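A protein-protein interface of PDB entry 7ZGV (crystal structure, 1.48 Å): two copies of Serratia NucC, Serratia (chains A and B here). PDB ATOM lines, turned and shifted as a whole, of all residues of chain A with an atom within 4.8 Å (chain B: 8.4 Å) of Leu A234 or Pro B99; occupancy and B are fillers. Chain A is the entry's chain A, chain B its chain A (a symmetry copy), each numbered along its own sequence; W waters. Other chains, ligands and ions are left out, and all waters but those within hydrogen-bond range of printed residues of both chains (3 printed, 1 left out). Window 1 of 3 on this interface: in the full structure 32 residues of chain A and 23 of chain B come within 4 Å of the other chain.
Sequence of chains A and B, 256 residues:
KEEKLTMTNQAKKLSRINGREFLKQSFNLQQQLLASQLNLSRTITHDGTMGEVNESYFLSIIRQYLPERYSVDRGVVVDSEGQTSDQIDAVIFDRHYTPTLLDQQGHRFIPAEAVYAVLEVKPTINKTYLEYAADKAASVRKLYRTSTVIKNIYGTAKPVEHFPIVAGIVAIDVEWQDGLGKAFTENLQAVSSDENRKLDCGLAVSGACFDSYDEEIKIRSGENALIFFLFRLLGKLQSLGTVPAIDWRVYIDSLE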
ATOM      1  N   TYR A  65      -0.457   5.336 -25.380  1.00  0.00           N
ATOM      2  CA  TYR A  65      -0.597   6.770 -25.236  1.00  0.00           C
ATOM      3  C   TYR A  65      -0.635   7.471 -26.583  1.00  0.00           C
ATOM      4  O   TYR A  65      -1.470   8.347 -26.808  1.00  0.00           O
ATOM      5  CB  TYR A  65       0.577   7.314 -24.411  1.00  0.00           C
ATOM      6  CG  TYR A  65       0.601   8.832 -24.348  1.00  0.00           C
ATOM      7  CD1 TYR A  65      -0.215   9.512 -23.488  1.00  0.00           C
ATOM      8  CD2 TYR A  65       1.445   9.566 -25.193  1.00  0.00           C
ATOM      9  CE1 TYR A  65      -0.220  10.916 -23.449  1.00  0.00           C
ATOM     10  CE2 TYR A  65       1.454  10.948 -25.166  1.00  0.00           C
ATOM     11  CZ  TYR A  65       0.619  11.612 -24.304  1.00  0.00           C
ATOM     12  OH  TYR A  65       0.615  12.991 -24.283  1.00  0.00           O
ATOM     13  N   LEU A  66       0.300   7.145 -27.471  1.00  0.00           N
ATOM     14  CA  LEU A  66       0.492   7.984 -28.646  1.00  0.00           C
ATOM     15  C   LEU A  66      -0.711   7.960 -29.589  1.00  0.00           C
ATOM     16  O   LEU A  66      -1.368   6.934 -29.751  1.00  0.00           O
ATOM     17  CB  LEU A  66       1.749   7.576 -29.426  1.00  0.00           C
ATOM     18  CG  LEU A  66       3.066   8.008 -28.764  1.00  0.00           C
ATOM     19  CD1 LEU A  66       4.175   7.405 -29.603  1.00  0.00           C
ATOM     20  CD2 LEU A  66       3.251   9.510 -28.650  1.00  0.00           C
ATOM     21  N   PRO A  67      -0.991   9.089 -30.235  1.00  0.00           N
ATOM     22  CA  PRO A  67      -1.993   9.125 -31.312  1.00  0.00           C
ATOM     23  C   PRO A  67      -1.745   8.037 -32.356  1.00  0.00           C
ATOM     24  O   PRO A  67      -0.605   7.630 -32.614  1.00  0.00           O
ATOM     25  CB  PRO A  67      -1.788  10.522 -31.909  1.00  0.00           C
ATOM     26  CG  PRO A  67      -1.267  11.360 -30.778  1.00  0.00           C
ATOM     27  CD  PRO A  67      -0.392  10.412 -29.981  1.00  0.00           C
ATOM     28  N   LEU A 230       5.721  12.029 -21.621  1.00  0.00           N
ATOM     29  CA  LEU A 230       4.823  11.675 -22.716  1.00  0.00           C
ATOM     30  C   LEU A 230       4.180  12.904 -23.344  1.00  0.00           C
ATOM     31  O   LEU A 230       4.098  12.992 -24.562  1.00  0.00           O
ATOM     32  CB  LEU A 230       3.784  10.675 -22.246  1.00  0.00           C
ATOM     33  CG  LEU A 230       4.301   9.272 -21.928  1.00  0.00           C
ATOM     34  CD1 LEU A 230       3.230   8.421 -21.296  1.00  0.00           C
ATOM     35  CD2 LEU A 230       4.868   8.588 -23.190  1.00  0.00           C
ATOM     36  N   PHE A 231       3.686  13.847 -22.549  1.00  0.00           N
ATOM     37  CA  PHE A 231       3.099  15.044 -23.138  1.00  0.00           C
ATOM     38  C   PHE A 231       4.145  15.906 -23.830  1.00  0.00           C
ATOM     39  O   PHE A 231       3.850  16.547 -24.843  1.00  0.00           O
ATOM     40  CB  PHE A 231       2.293  15.854 -22.109  1.00  0.00           C
ATOM     41  CG  PHE A 231       0.866  15.356 -21.966  1.00  0.00           C
ATOM     42  CD1 PHE A 231       0.570  14.311 -21.112  1.00  0.00           C
ATOM     43  CD2 PHE A 231      -0.136  15.863 -22.755  1.00  0.00           C
ATOM     44  CE1 PHE A 231      -0.746  13.831 -21.016  1.00  0.00           C
ATOM     45  CE2 PHE A 231      -1.444  15.374 -22.682  1.00  0.00           C
ATOM     46  CZ  PHE A 231      -1.743  14.383 -21.774  1.00  0.00           C
ATOM     47  N   ARG A 232       5.355  16.009 -23.262  1.00  0.00           N
ATOM     48  CA  ARG A 232       6.378  16.807 -23.927  1.00  0.00           C
ATOM     49  C   ARG A 232       6.774  16.142 -25.237  1.00  0.00           C
ATOM     50  O   ARG A 232       6.936  16.822 -26.246  1.00  0.00           O
ATOM     51  CB  ARG A 232       7.585  17.023 -22.998  1.00  0.00           C
ATOM     52  CG  ARG A 232       7.217  17.718 -21.688  1.00  0.00           C
ATOM     53  CD  ARG A 232       7.462  19.161 -21.730  1.00  0.00           C
ATOM     54  NE  ARG A 232       8.819  19.548 -22.117  1.00  0.00           N
ATOM     55  CZ  ARG A 232       9.090  20.773 -22.538  1.00  0.00           C
ATOM     56  NH1 ARG A 232       8.172  21.725 -22.507  1.00  0.00           N
ATOM     57  NH2 ARG A 232      10.291  21.048 -23.023  1.00  0.00           N
ATOM     58  N   LEU A 233       6.844  14.807 -25.255  1.00  0.00           N
ATOM     59  CA  LEU A 233       7.166  14.107 -26.502  1.00  0.00           C
ATOM     60  C   LEU A 233       6.061  14.299 -27.512  1.00  0.00           C
ATOM     61  O   LEU A 233       6.334  14.504 -28.709  1.00  0.00           O
ATOM     62  CB  LEU A 233       7.368  12.629 -26.215  1.00  0.00           C
ATOM     63  CG  LEU A 233       7.576  11.726 -27.443  1.00  0.00           C
ATOM     64  CD1 LEU A 233       8.824  12.097 -28.123  1.00  0.00           C
ATOM     65  CD2 LEU A 233       7.592  10.266 -27.032  1.00  0.00           C
ATOM     66  N   LEU A 234       4.805  14.199 -27.060  1.00  0.00           N
ATOM     67  CA  LEU A 234       3.674  14.483 -27.944  1.00  0.00           C
ATOM     68  C   LEU A 234       3.846  15.829 -28.632  1.00  0.00           C
ATOM     69  O   LEU A 234       3.614  15.954 -29.846  1.00  0.00           O
ATOM     70  CB  LEU A 234       2.372  14.486 -27.133  1.00  0.00           C
ATOM     71  CG  LEU A 234       1.088  14.873 -27.877  1.00  0.00           C
ATOM     72  CD1 LEU A 234       0.654  13.697 -28.728  1.00  0.00           C
ATOM     73  CD2 LEU A 234      -0.029  15.278 -26.911  1.00  0.00           C
ATOM     74  N   GLY A 235       4.184  16.870 -27.856  1.00  0.00           N
ATOM     75  CA  GLY A 235       4.371  18.183 -28.430  1.00  0.00           C
ATOM     76  C   GLY A 235       5.516  18.239 -29.412  1.00  0.00           C
ATOM     77  O   GLY A 235       5.430  18.914 -30.435  1.00  0.00           O
ATOM     78  N   LYS A 236       6.630  17.601 -29.079  1.00  0.00           N
ATOM     79  CA  LYS A 236       7.741  17.596 -30.009  1.00  0.00           C
ATOM     80  C   LYS A 236       7.338  16.913 -31.311  1.00  0.00           C
ATOM     81  O   LYS A 236       7.539  17.466 -32.387  1.00  0.00           O
ATOM     82  CB  LYS A 236       8.958  16.906 -29.390  1.00  0.00           C
ATOM     83  CG  LYS A 236      10.171  16.802 -30.350  1.00  0.00           C
ATOM     84  CD  LYS A 236      10.673  18.187 -30.729  1.00  0.00           C
ATOM     85  CE  LYS A 236      11.944  18.112 -31.557  1.00  0.00           C
ATOM     86  NZ  LYS A 236      12.442  19.478 -31.871  1.00  0.00           N
ATOM     87  N   LEU A 237       6.709  15.732 -31.220  1.00  0.00           N
ATOM     88  CA  LEU A 237       6.193  15.048 -32.403  1.00  0.00           C
ATOM     89  C   LEU A 237       5.241  15.926 -33.186  1.00  0.00           C
ATOM     90  O   LEU A 237       5.319  15.981 -34.420  1.00  0.00           O
ATOM     91  CB  LEU A 237       5.530  13.733 -32.017  1.00  0.00           C
ATOM     92  CG  LEU A 237       6.481  12.663 -31.499  1.00  0.00           C
ATOM     93  CD1 LEU A 237       5.649  11.539 -30.935  1.00  0.00           C
ATOM     94  CD2 LEU A 237       7.465  12.119 -32.569  1.00  0.00           C
ATOM     95  N   GLN A 238       4.319  16.610 -32.493  1.00  0.00           N
ATOM     96  CA  GLN A 238       3.376  17.496 -33.164  1.00  0.00           C
ATOM     97  C   GLN A 238       4.106  18.458 -34.071  1.00  0.00           C
ATOM     98  O   GLN A 238       3.677  18.715 -35.202  1.00  0.00           O
ATOM     99  CB  GLN A 238       2.607  18.322 -32.130  1.00  0.00           C
ATOM    100  CG  GLN A 238       1.214  18.000 -31.958  1.00  0.00           C
ATOM    101  CD  GLN A 238       0.560  18.916 -30.947  1.00  0.00           C
ATOM    102  OE1 GLN A 238       1.224  19.670 -30.226  1.00  0.00           O
ATOM    103  NE2 GLN A 238      -0.738  18.864 -30.897  1.00  0.00           N
ATOM    104  N   PHE B  93     -15.046  10.342 -31.262  1.00  0.00           N
ATOM    105  CA  PHE B  93     -13.890  11.150 -30.898  1.00  0.00           C
ATOM    106  C   PHE B  93     -12.678  10.773 -31.738  1.00  0.00           C
ATOM    107  O   PHE B  93     -12.660   9.746 -32.405  1.00  0.00           O
ATOM    108  CB  PHE B  93     -13.576  11.060 -29.402  1.00  0.00           C
ATOM    109  CG  PHE B  93     -13.168   9.677 -28.907  1.00  0.00           C
ATOM    110  CD1 PHE B  93     -14.105   8.655 -28.756  1.00  0.00           C
ATOM    111  CD2 PHE B  93     -11.842   9.416 -28.544  1.00  0.00           C
ATOM    112  CE1 PHE B  93     -13.737   7.410 -28.272  1.00  0.00           C
ATOM    113  CE2 PHE B  93     -11.468   8.162 -28.060  1.00  0.00           C
ATOM    114  CZ  PHE B  93     -12.392   7.156 -27.933  1.00  0.00           C
ATOM    115  N   ASP B  94     -11.669  11.633 -31.699  1.00  0.00           N
ATOM    116  CA  ASP B  94     -10.410  11.386 -32.396  1.00  0.00           C
ATOM    117  C   ASP B  94      -9.365  10.692 -31.532  1.00  0.00           C
ATOM    118  O   ASP B  94      -9.115  11.090 -30.382  1.00  0.00           O
ATOM    119  CB  ASP B  94      -9.788  12.709 -32.833  1.00  0.00           C
ATOM    120  CG  ASP B  94      -8.420  12.492 -33.463  1.00  0.00           C
ATOM    121  OD1 ASP B  94      -8.374  11.904 -34.575  1.00  0.00           O
ATOM    122  OD2 ASP B  94      -7.415  12.875 -32.851  1.00  0.00           O
ATOM    123  N   ARG B  95      -8.706   9.710 -32.133  1.00  0.00           N
ATOM    124  CA  ARG B  95      -7.492   9.116 -31.602  1.00  0.00           C
ATOM    125  C   ARG B  95      -6.365   9.154 -32.614  1.00  0.00           C
ATOM    126  O   ARG B  95      -5.252   8.738 -32.277  1.00  0.00           O
ATOM    127  CB  ARG B  95      -7.708   7.656 -31.176  1.00  0.00           C
ATOM    128  CG  ARG B  95      -8.661   7.506 -29.995  1.00  0.00           C
ATOM    129  CD  ARG B  95      -8.929   6.036 -29.686  1.00  0.00           C
ATOM    130  NE  ARG B  95      -7.736   5.380 -29.186  1.00  0.00           N
ATOM    131  CZ  ARG B  95      -7.534   4.072 -29.233  1.00  0.00           C
ATOM    132  NH1 ARG B  95      -8.416   3.257 -29.795  1.00  0.00           N
ATOM    133  NH2 ARG B  95      -6.418   3.569 -28.705  1.00  0.00           N
ATOM    134  N   HIS B  96      -6.603   9.649 -33.835  1.00  0.00           N
ATOM    135  CA  HIS B  96      -5.523   9.682 -34.822  1.00  0.00           C
ATOM    136  C   HIS B  96      -4.490  10.762 -34.501  1.00  0.00           C
ATOM    137  O   HIS B  96      -3.288  10.555 -34.729  1.00  0.00           O
ATOM    138  CB  HIS B  96      -6.146   9.888 -36.218  1.00  0.00           C
ATOM    139  CG  HIS B  96      -5.208   9.650 -37.351  1.00  0.00           C
ATOM    140  ND1 HIS B  96      -4.874   8.389 -37.800  1.00  0.00           N
ATOM    141  CD2 HIS B  96      -4.495  10.528 -38.093  1.00  0.00           C
ATOM    142  CE1 HIS B  96      -4.007   8.511 -38.797  1.00  0.00           C
ATOM    143  NE2 HIS B  96      -3.773   9.799 -39.001  1.00  0.00           N
ATOM    144  N   TYR B  97      -4.926  11.906 -33.946  1.00  0.00           N
ATOM    145  CA  TYR B  97      -4.062  13.036 -33.626  1.00  0.00           C
ATOM    146  C   TYR B  97      -3.980  13.335 -32.154  1.00  0.00           C
ATOM    147  O   TYR B  97      -3.072  14.053 -31.751  1.00  0.00           O
ATOM    148  CB  TYR B  97      -4.578  14.314 -34.317  1.00  0.00           C
ATOM    149  CG  TYR B  97      -4.512  14.193 -35.815  1.00  0.00           C
ATOM    150  CD1 TYR B  97      -3.290  14.305 -36.457  1.00  0.00           C
ATOM    151  CD2 TYR B  97      -5.646  13.966 -36.590  1.00  0.00           C
ATOM    152  CE1 TYR B  97      -3.189  14.170 -37.829  1.00  0.00           C
ATOM    153  CE2 TYR B  97      -5.557  13.852 -37.972  1.00  0.00           C
ATOM    154  CZ  TYR B  97      -4.324  13.959 -38.570  1.00  0.00           C
ATOM    155  OH  TYR B  97      -4.162  13.848 -39.929  1.00  0.00           O
ATOM    156  N   THR B  98      -4.863  12.790 -31.357  1.00  0.00           N
ATOM    157  CA  THR B  98      -5.024  13.133 -29.966  1.00  0.00           C
ATOM    158  C   THR B  98      -4.642  11.930 -29.136  1.00  0.00           C
ATOM    159  O   THR B  98      -5.077  10.816 -29.446  1.00  0.00           O
ATOM    160  CB  THR B  98      -6.504  13.508 -29.732  1.00  0.00           C
ATOM    161  OG1 THR B  98      -6.926  14.460 -30.701  1.00  0.00           O
ATOM    162  CG2 THR B  98      -6.680  14.193 -28.377  1.00  0.00           C
ATOM    163  N   PRO B  99      -3.812  12.097 -28.091  1.00  0.00           N
ATOM    164  CA  PRO B  99      -3.366  10.951 -27.303  1.00  0.00           C
ATOM    165  C   PRO B  99      -4.489  10.325 -26.501  1.00  0.00           C
ATOM    166  O   PRO B  99      -5.561  10.904 -26.297  1.00  0.00           O
ATOM    167  CB  PRO B  99      -2.359  11.583 -26.336  1.00  0.00           C
ATOM    168  CG  PRO B  99      -2.902  12.950 -26.118  1.00  0.00           C
ATOM    169  CD  PRO B  99      -3.365  13.368 -27.497  1.00  0.00           C
ATOM    170  N   THR B 100      -4.201   9.118 -26.023  1.00  0.00           N
ATOM    171  CA  THR B 100      -5.078   8.344 -25.156  1.00  0.00           C
ATOM    172  C   THR B 100      -4.493   8.360 -23.756  1.00  0.00           C
ATOM    173  O   THR B 100      -3.301   8.085 -23.584  1.00  0.00           O
ATOM    174  CB  THR B 100      -5.141   6.916 -25.704  1.00  0.00           C
ATOM    175  OG1 THR B 100      -5.932   6.889 -26.898  1.00  0.00           O
ATOM    176  CG2 THR B 100      -5.689   5.939 -24.705  1.00  0.00           C
ATOM    177  N   LEU B 101      -5.330   8.667 -22.764  1.00  0.00           N
ATOM    178  CA  LEU B 101      -4.911   8.887 -21.389  1.00  0.00           C
ATOM    179  C   LEU B 101      -4.806   7.577 -20.616  1.00  0.00           C
ATOM    180  O   LEU B 101      -5.181   7.472 -19.435  1.00  0.00           O
ATOM    181  CB  LEU B 101      -5.833   9.894 -20.707  1.00  0.00           C
ATOM    182  CG  LEU B 101      -6.002  11.238 -21.434  1.00  0.00           C
ATOM    183  CD1 LEU B 101      -6.862  12.209 -20.622  1.00  0.00           C
ATOM    184  CD2 LEU B 101      -4.620  11.825 -21.798  1.00  0.00           C
ATOM    185  N   LEU B 102      -4.186   6.594 -21.276  1.00  0.00           N
ATOM    186  CA  LEU B 102      -3.861   5.309 -20.689  1.00  0.00           C
ATOM    187  C   LEU B 102      -5.115   4.624 -20.162  1.00  0.00           C
ATOM    188  O   LEU B 102      -5.125   4.010 -19.093  1.00  0.00           O
ATOM    189  CB  LEU B 102      -2.737   5.435 -19.642  1.00  0.00           C
ATOM    190  CG  LEU B 102      -1.417   5.959 -20.184  1.00  0.00           C
ATOM    191  CD1 LEU B 102      -0.307   5.919 -19.131  1.00  0.00           C
ATOM    192  CD2 LEU B 102      -0.990   5.166 -21.392  1.00  0.00           C
ATOM    193  N   ASP B 103      -6.152   4.670 -20.974  1.00  0.00           N
ATOM    194  CA  ASP B 103      -7.399   3.994 -20.688  1.00  0.00           C
ATOM    195  C   ASP B 103      -7.515   2.773 -21.600  1.00  0.00           C
ATOM    196  O   ASP B 103      -6.567   2.392 -22.313  1.00  0.00           O
ATOM    197  CB  ASP B 103      -8.548   4.998 -20.809  1.00  0.00           C
ATOM    198  CG  ASP B 103      -8.660   5.589 -22.193  1.00  0.00           C
ATOM    199  OD1 ASP B 103      -8.075   5.005 -23.127  1.00  0.00           O
ATOM    200  OD2 ASP B 103      -9.323   6.630 -22.397  1.00  0.00           O
ATOM    201  N   PHE B 109     -11.333   7.878 -20.837  1.00  0.00           N
ATOM    202  CA  PHE B 109     -11.168   9.148 -20.120  1.00  0.00           C
ATOM    203  C   PHE B 109     -10.592  10.058 -21.200  1.00  0.00           C
ATOM    204  O   PHE B 109      -9.394  10.023 -21.462  1.00  0.00           O
ATOM    205  CB  PHE B 109     -10.211   8.911 -18.956  1.00  0.00           C
ATOM    206  CG  PHE B 109     -10.010  10.094 -18.031  1.00  0.00           C
ATOM    207  CD1 PHE B 109     -11.074  10.607 -17.291  1.00  0.00           C
ATOM    208  CD2 PHE B 109      -8.739  10.632 -17.850  1.00  0.00           C
ATOM    209  CE1 PHE B 109     -10.882  11.656 -16.398  1.00  0.00           C
ATOM    210  CE2 PHE B 109      -8.542  11.692 -16.964  1.00  0.00           C
ATOM    211  CZ  PHE B 109      -9.634  12.195 -16.253  1.00  0.00           C
ATOM    212  N   ILE B 110     -11.435  10.848 -21.846  1.00  0.00           N
ATOM    213  CA  ILE B 110     -11.170  11.414 -23.167  1.00  0.00           C
ATOM    214  C   ILE B 110     -10.901  12.912 -23.043  1.00  0.00           C
ATOM    215  O   ILE B 110     -11.762  13.637 -22.533  1.00  0.00           O
ATOM    216  CB  ILE B 110     -12.364  11.171 -24.118  1.00  0.00           C
ATOM    217  CG1 ILE B 110     -12.619   9.662 -24.255  1.00  0.00           C
ATOM    218  CG2 ILE B 110     -12.089  11.765 -25.465  1.00  0.00           C
ATOM    219  CD1 ILE B 110     -13.872   9.317 -24.997  1.00  0.00           C
ATOM    220  N   PRO B 111      -9.808  13.440 -23.611  1.00  0.00           N
ATOM    221  CA  PRO B 111      -9.632  14.903 -23.643  1.00  0.00           C
ATOM    222  C   PRO B 111     -10.735  15.571 -24.447  1.00  0.00           C
ATOM    223  O   PRO B 111     -11.081  15.129 -25.548  1.00  0.00           O
ATOM    224  CB  PRO B 111      -8.263  15.100 -24.320  1.00  0.00           C
ATOM    225  CG  PRO B 111      -7.630  13.790 -24.397  1.00  0.00           C
ATOM    226  CD  PRO B 111      -8.705  12.738 -24.274  1.00  0.00           C
ATOM    227  N   GLU B 113     -10.818  18.075 -26.288  1.00  0.00           N
ATOM    228  CA  GLU B 113     -10.439  18.438 -27.649  1.00  0.00           C
ATOM    229  C   GLU B 113     -10.700  17.330 -28.663  1.00  0.00           C
ATOM    230  O   GLU B 113     -10.817  17.612 -29.853  1.00  0.00           O
ATOM    231  CB  GLU B 113      -8.939  18.772 -27.674  1.00  0.00           C
ATOM    232  CG  GLU B 113      -8.524  20.078 -26.991  1.00  0.00           C
ATOM    233  CD  GLU B 113      -8.323  19.939 -25.494  1.00  0.00           C
ATOM    234  OE1 GLU B 113      -8.593  18.855 -24.894  1.00  0.00           O
ATOM    235  OE2 GLU B 113      -7.890  20.964 -24.878  1.00  0.00           O
ATOM    236  N   ALA B 114     -10.739  16.082 -28.230  1.00  0.00           N
ATOM    237  CA  ALA B 114     -10.907  14.973 -29.161  1.00  0.00           C
ATOM    238  C   ALA B 114     -12.350  14.758 -29.605  1.00  0.00           C
ATOM    239  O   ALA B 114     -12.578  13.948 -30.500  1.00  0.00           O
ATOM    240  CB  ALA B 114     -10.481  13.692 -28.477  1.00  0.00           C
ATOM    241  N   ALA B 245      -5.816  20.892 -33.152  1.00  0.00           N
ATOM    242  CA  ALA B 245      -4.622  20.345 -32.523  1.00  0.00           C
ATOM    243  C   ALA B 245      -4.583  20.741 -31.052  1.00  0.00           C
ATOM    244  O   ALA B 245      -4.562  21.931 -30.716  1.00  0.00           O
ATOM    245  CB  ALA B 245      -3.375  20.843 -33.230  1.00  0.00           C
ATOM    246  N   ILE B 246      -4.556  19.726 -30.190  1.00  0.00           N
ATOM    247  CA  ILE B 246      -4.541  19.913 -28.752  1.00  0.00           C
ATOM    248  C   ILE B 246      -3.267  20.639 -28.336  1.00  0.00           C
ATOM    249  O   ILE B 246      -2.179  20.396 -28.869  1.00  0.00           O
ATOM    250  CB  ILE B 246      -4.682  18.521 -28.110  1.00  0.00           C
ATOM    251  CG1 ILE B 246      -4.801  18.623 -26.595  1.00  0.00           C
ATOM    252  CG2 ILE B 246      -3.495  17.568 -28.510  1.00  0.00           C
ATOM    253  CD1 ILE B 246      -5.127  17.256 -25.940  1.00  0.00           C
ATOM    254  N   ASP B 247      -3.402  21.564 -27.383  1.00  0.00           N
ATOM    255  CA  ASP B 247      -2.251  22.180 -26.725  1.00  0.00           C
ATOM    256  C   ASP B 247      -1.761  21.230 -25.641  1.00  0.00           C
ATOM    257  O   ASP B 247      -2.364  21.126 -24.571  1.00  0.00           O
ATOM    258  CB  ASP B 247      -2.635  23.526 -26.118  1.00  0.00           C
ATOM    259  CG  ASP B 247      -1.439  24.288 -25.573  1.00  0.00           C
ATOM    260  OD1 ASP B 247      -0.346  23.690 -25.541  1.00  0.00           O
ATOM    261  OD2 ASP B 247      -1.583  25.459 -25.172  1.00  0.00           O
ATOM    262  N   TRP B 248      -0.661  20.545 -25.919  1.00  0.00           N
ATOM    263  CA  TRP B 248      -0.126  19.575 -24.974  1.00  0.00           C
ATOM    264  C   TRP B 248       0.314  20.223 -23.667  1.00  0.00           C
ATOM    265  O   TRP B 248       0.373  19.546 -22.638  1.00  0.00           O
ATOM    266  CB  TRP B 248       1.047  18.840 -25.636  1.00  0.00           C
ATOM    267  CG  TRP B 248       2.087  19.766 -26.129  1.00  0.00           C
ATOM    268  CD1 TRP B 248       2.171  20.327 -27.382  1.00  0.00           C
ATOM    269  CD2 TRP B 248       3.179  20.308 -25.373  1.00  0.00           C
ATOM    270  NE1 TRP B 248       3.258  21.159 -27.441  1.00  0.00           N
ATOM    271  CE2 TRP B 248       3.892  21.171 -26.224  1.00  0.00           C
ATOM    272  CE3 TRP B 248       3.633  20.134 -24.057  1.00  0.00           C
ATOM    273  CZ2 TRP B 248       5.018  21.857 -25.802  1.00  0.00           C
ATOM    274  CZ3 TRP B 248       4.733  20.809 -23.645  1.00  0.00           C
ATOM    275  CH2 TRP B 248       5.428  21.672 -24.511  1.00  0.00           C
ATOM    276  N   ARG B 249       0.617  21.517 -23.669  1.00  0.00           N
ATOM    277  CA  ARG B 249       1.117  22.155 -22.459  1.00  0.00           C
ATOM    278  C   ARG B 249       0.069  22.194 -21.348  1.00  0.00           C
ATOM    279  O   ARG B 249       0.423  22.200 -20.161  1.00  0.00           O
ATOM    280  CB  ARG B 249       1.501  23.593 -22.790  1.00  0.00           C
ATOM    281  CG  ARG B 249       2.553  23.703 -23.901  1.00  0.00           C
ATOM    282  CD  ARG B 249       2.659  25.117 -24.499  1.00  0.00           C
ATOM    283  NE  ARG B 249       3.457  25.105 -25.727  1.00  0.00           N
ATOM    284  CZ  ARG B 249       3.007  24.754 -26.929  1.00  0.00           C
ATOM    285  NH1 ARG B 249       1.733  24.447 -27.140  1.00  0.00           N
ATOM    286  NH2 ARG B 249       3.865  24.689 -27.950  1.00  0.00           N
ATOM    287  N   TYR B 251      -2.296  20.187 -20.286  1.00  0.00           N
ATOM    288  CA  TYR B 251      -2.570  19.003 -19.491  1.00  0.00           C
ATOM    289  C   TYR B 251      -1.473  18.694 -18.479  1.00  0.00           C
ATOM    290  O   TYR B 251      -1.627  17.758 -17.689  1.00  0.00           O
ATOM    291  CB  TYR B 251      -2.845  17.810 -20.409  1.00  0.00           C
ATOM    292  CG  TYR B 251      -4.257  17.883 -20.966  1.00  0.00           C
ATOM    293  CD1 TYR B 251      -5.310  17.322 -20.266  1.00  0.00           C
ATOM    294  CD2 TYR B 251      -4.533  18.520 -22.179  1.00  0.00           C
ATOM    295  CE1 TYR B 251      -6.617  17.403 -20.746  1.00  0.00           C
ATOM    296  CE2 TYR B 251      -5.858  18.599 -22.656  1.00  0.00           C
ATOM    297  CZ  TYR B 251      -6.867  18.027 -21.922  1.00  0.00           C
ATOM    298  OH  TYR B 251      -8.158  18.091 -22.370  1.00  0.00           O
HETATM  299  O   HOH W   1       0.434  22.279 -29.266  1.00  0.00           O
HETATM  300  O   HOH W   2       4.450  21.465 -30.343  1.00  0.00           O
HETATM  301  O   HOH W   3      -2.253  16.914 -32.554  1.00  0.00           O
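O of Tyr A65 lies within hydrogen-bond range of N of Thr B100, at 2.9 Å. O of Ile B246 lies within hydrogen-bond range of NE2 of Gln A238 (2.9 Å).
The side-chain hydroxyl of Tyr A65 lies close to the backbone carbonyl oxygen of Leu A230. The backbone NH (N) of His B96 lies within hydrogen-bond range of the side-chain carboxylate (OD1) of Asp B94 (3.0 Å). The side-chain carboxylate (OD2) of Asp B94 lies within hydrogen-bond range of the backbone NH (N) of Tyr B97, at 2.9 Å. The side-chain hydroxyl (OG1) of Thr B98 is in hydrogen-bond range of the side-chain carboxylate (OD2) of Asp B94. The side-chain hydroxyl of Thr B100 sits at hydrogen-bond distance from the guanidinium group of Arg B95 (3.3 Å). OH of Tyr B251 lies within hydrogen-bond range of OE1 of Glu B113, at 2.7 Å.
Among the printed residues, merely in contact across the chains: Gln A238 with Trp B248 (3.1 Å), Pro A67 with His B96 (3.2 Å), Gly A235 with Trp B248 (3.2 Å), Tyr A65 with Pro B99 (3.3 Å), Pro A67 with Tyr B97 (3.4 Å), Arg A232 with Trp B248 (3.4 Å), Pro A67 with Arg B95 (3.4 Å), Phe A231 with Tyr B251 (3.6 Å), Phe A231 with Trp B248 (3.7 Å), Pro A67 with Pro B99 (3.8 Å), Leu A234 with Pro B99 (3.8 Å), Pro A67 with Thr B98 (3.8 Å), Phe A231 with Leu B101 (3.8 Å) and Leu A234 with Trp B248 (3.9 Å).
Leu A234 touches two residues of chain B. Of chain A, only Tyr A65 (3.3 Å), Pro A67 (3.8 Å) and Leu A234 (3.8 Å) come within 4 Å of Pro B99. Of the printed residues of chain B, Phe A231 touches Leu B101 (3.8 Å), Trp B248 (3.7 Å) and Tyr B251 (3.6 Å). Printed residues of chain A within 4 Å of Tyr B97: Pro A67 (3.4 Å). Of the printed residues of chain A, Leu B101 touches Phe A231. Of the printed residues of chain A, Thr B100 touches Tyr A65. The nearest residue of chain A that does not touch Pro B99 is Phe A231 (4.5 Å). The nearest printed residue of chain A that does not touch His B96 is Leu A66 (6.3 Å).
Of the 12 printed residues of chain A, 7 touch a printed residue of chain B. Printed residues of chain A that touch a printed residue of chain B: Tyr A65, Pro A67, Phe A231, Arg A232, Leu A234, Gly A235 and Gln A238. Of the 22 printed residues of chain B, 10 touch a printed residue of chain A. Printed residues of chain B that touch a printed residue of chain A: Arg B95, His B96, Tyr B97, Thr B98, Pro B99, Thr B100, Leu B101, Ile B246, Trp B248 and Tyr B251. Among the printed residues, 16 pairs touch across the chains.
No position is printed for both chains. Of the 16 pairs that touch across the chains among the printed residues, none has its exchanged pair printed and touching as well.
Water W2 lies within hydrogen-bond range of O of Gly A235 and NE1 of Trp B248. Water W1 lies within hydrogen-bond range of OE1 of Gln A238, O of Ile B246 and NH1 of Arg B249. Water W3 lies within hydrogen-bond range of NE2 of Gln A238 and O of Tyr B97.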
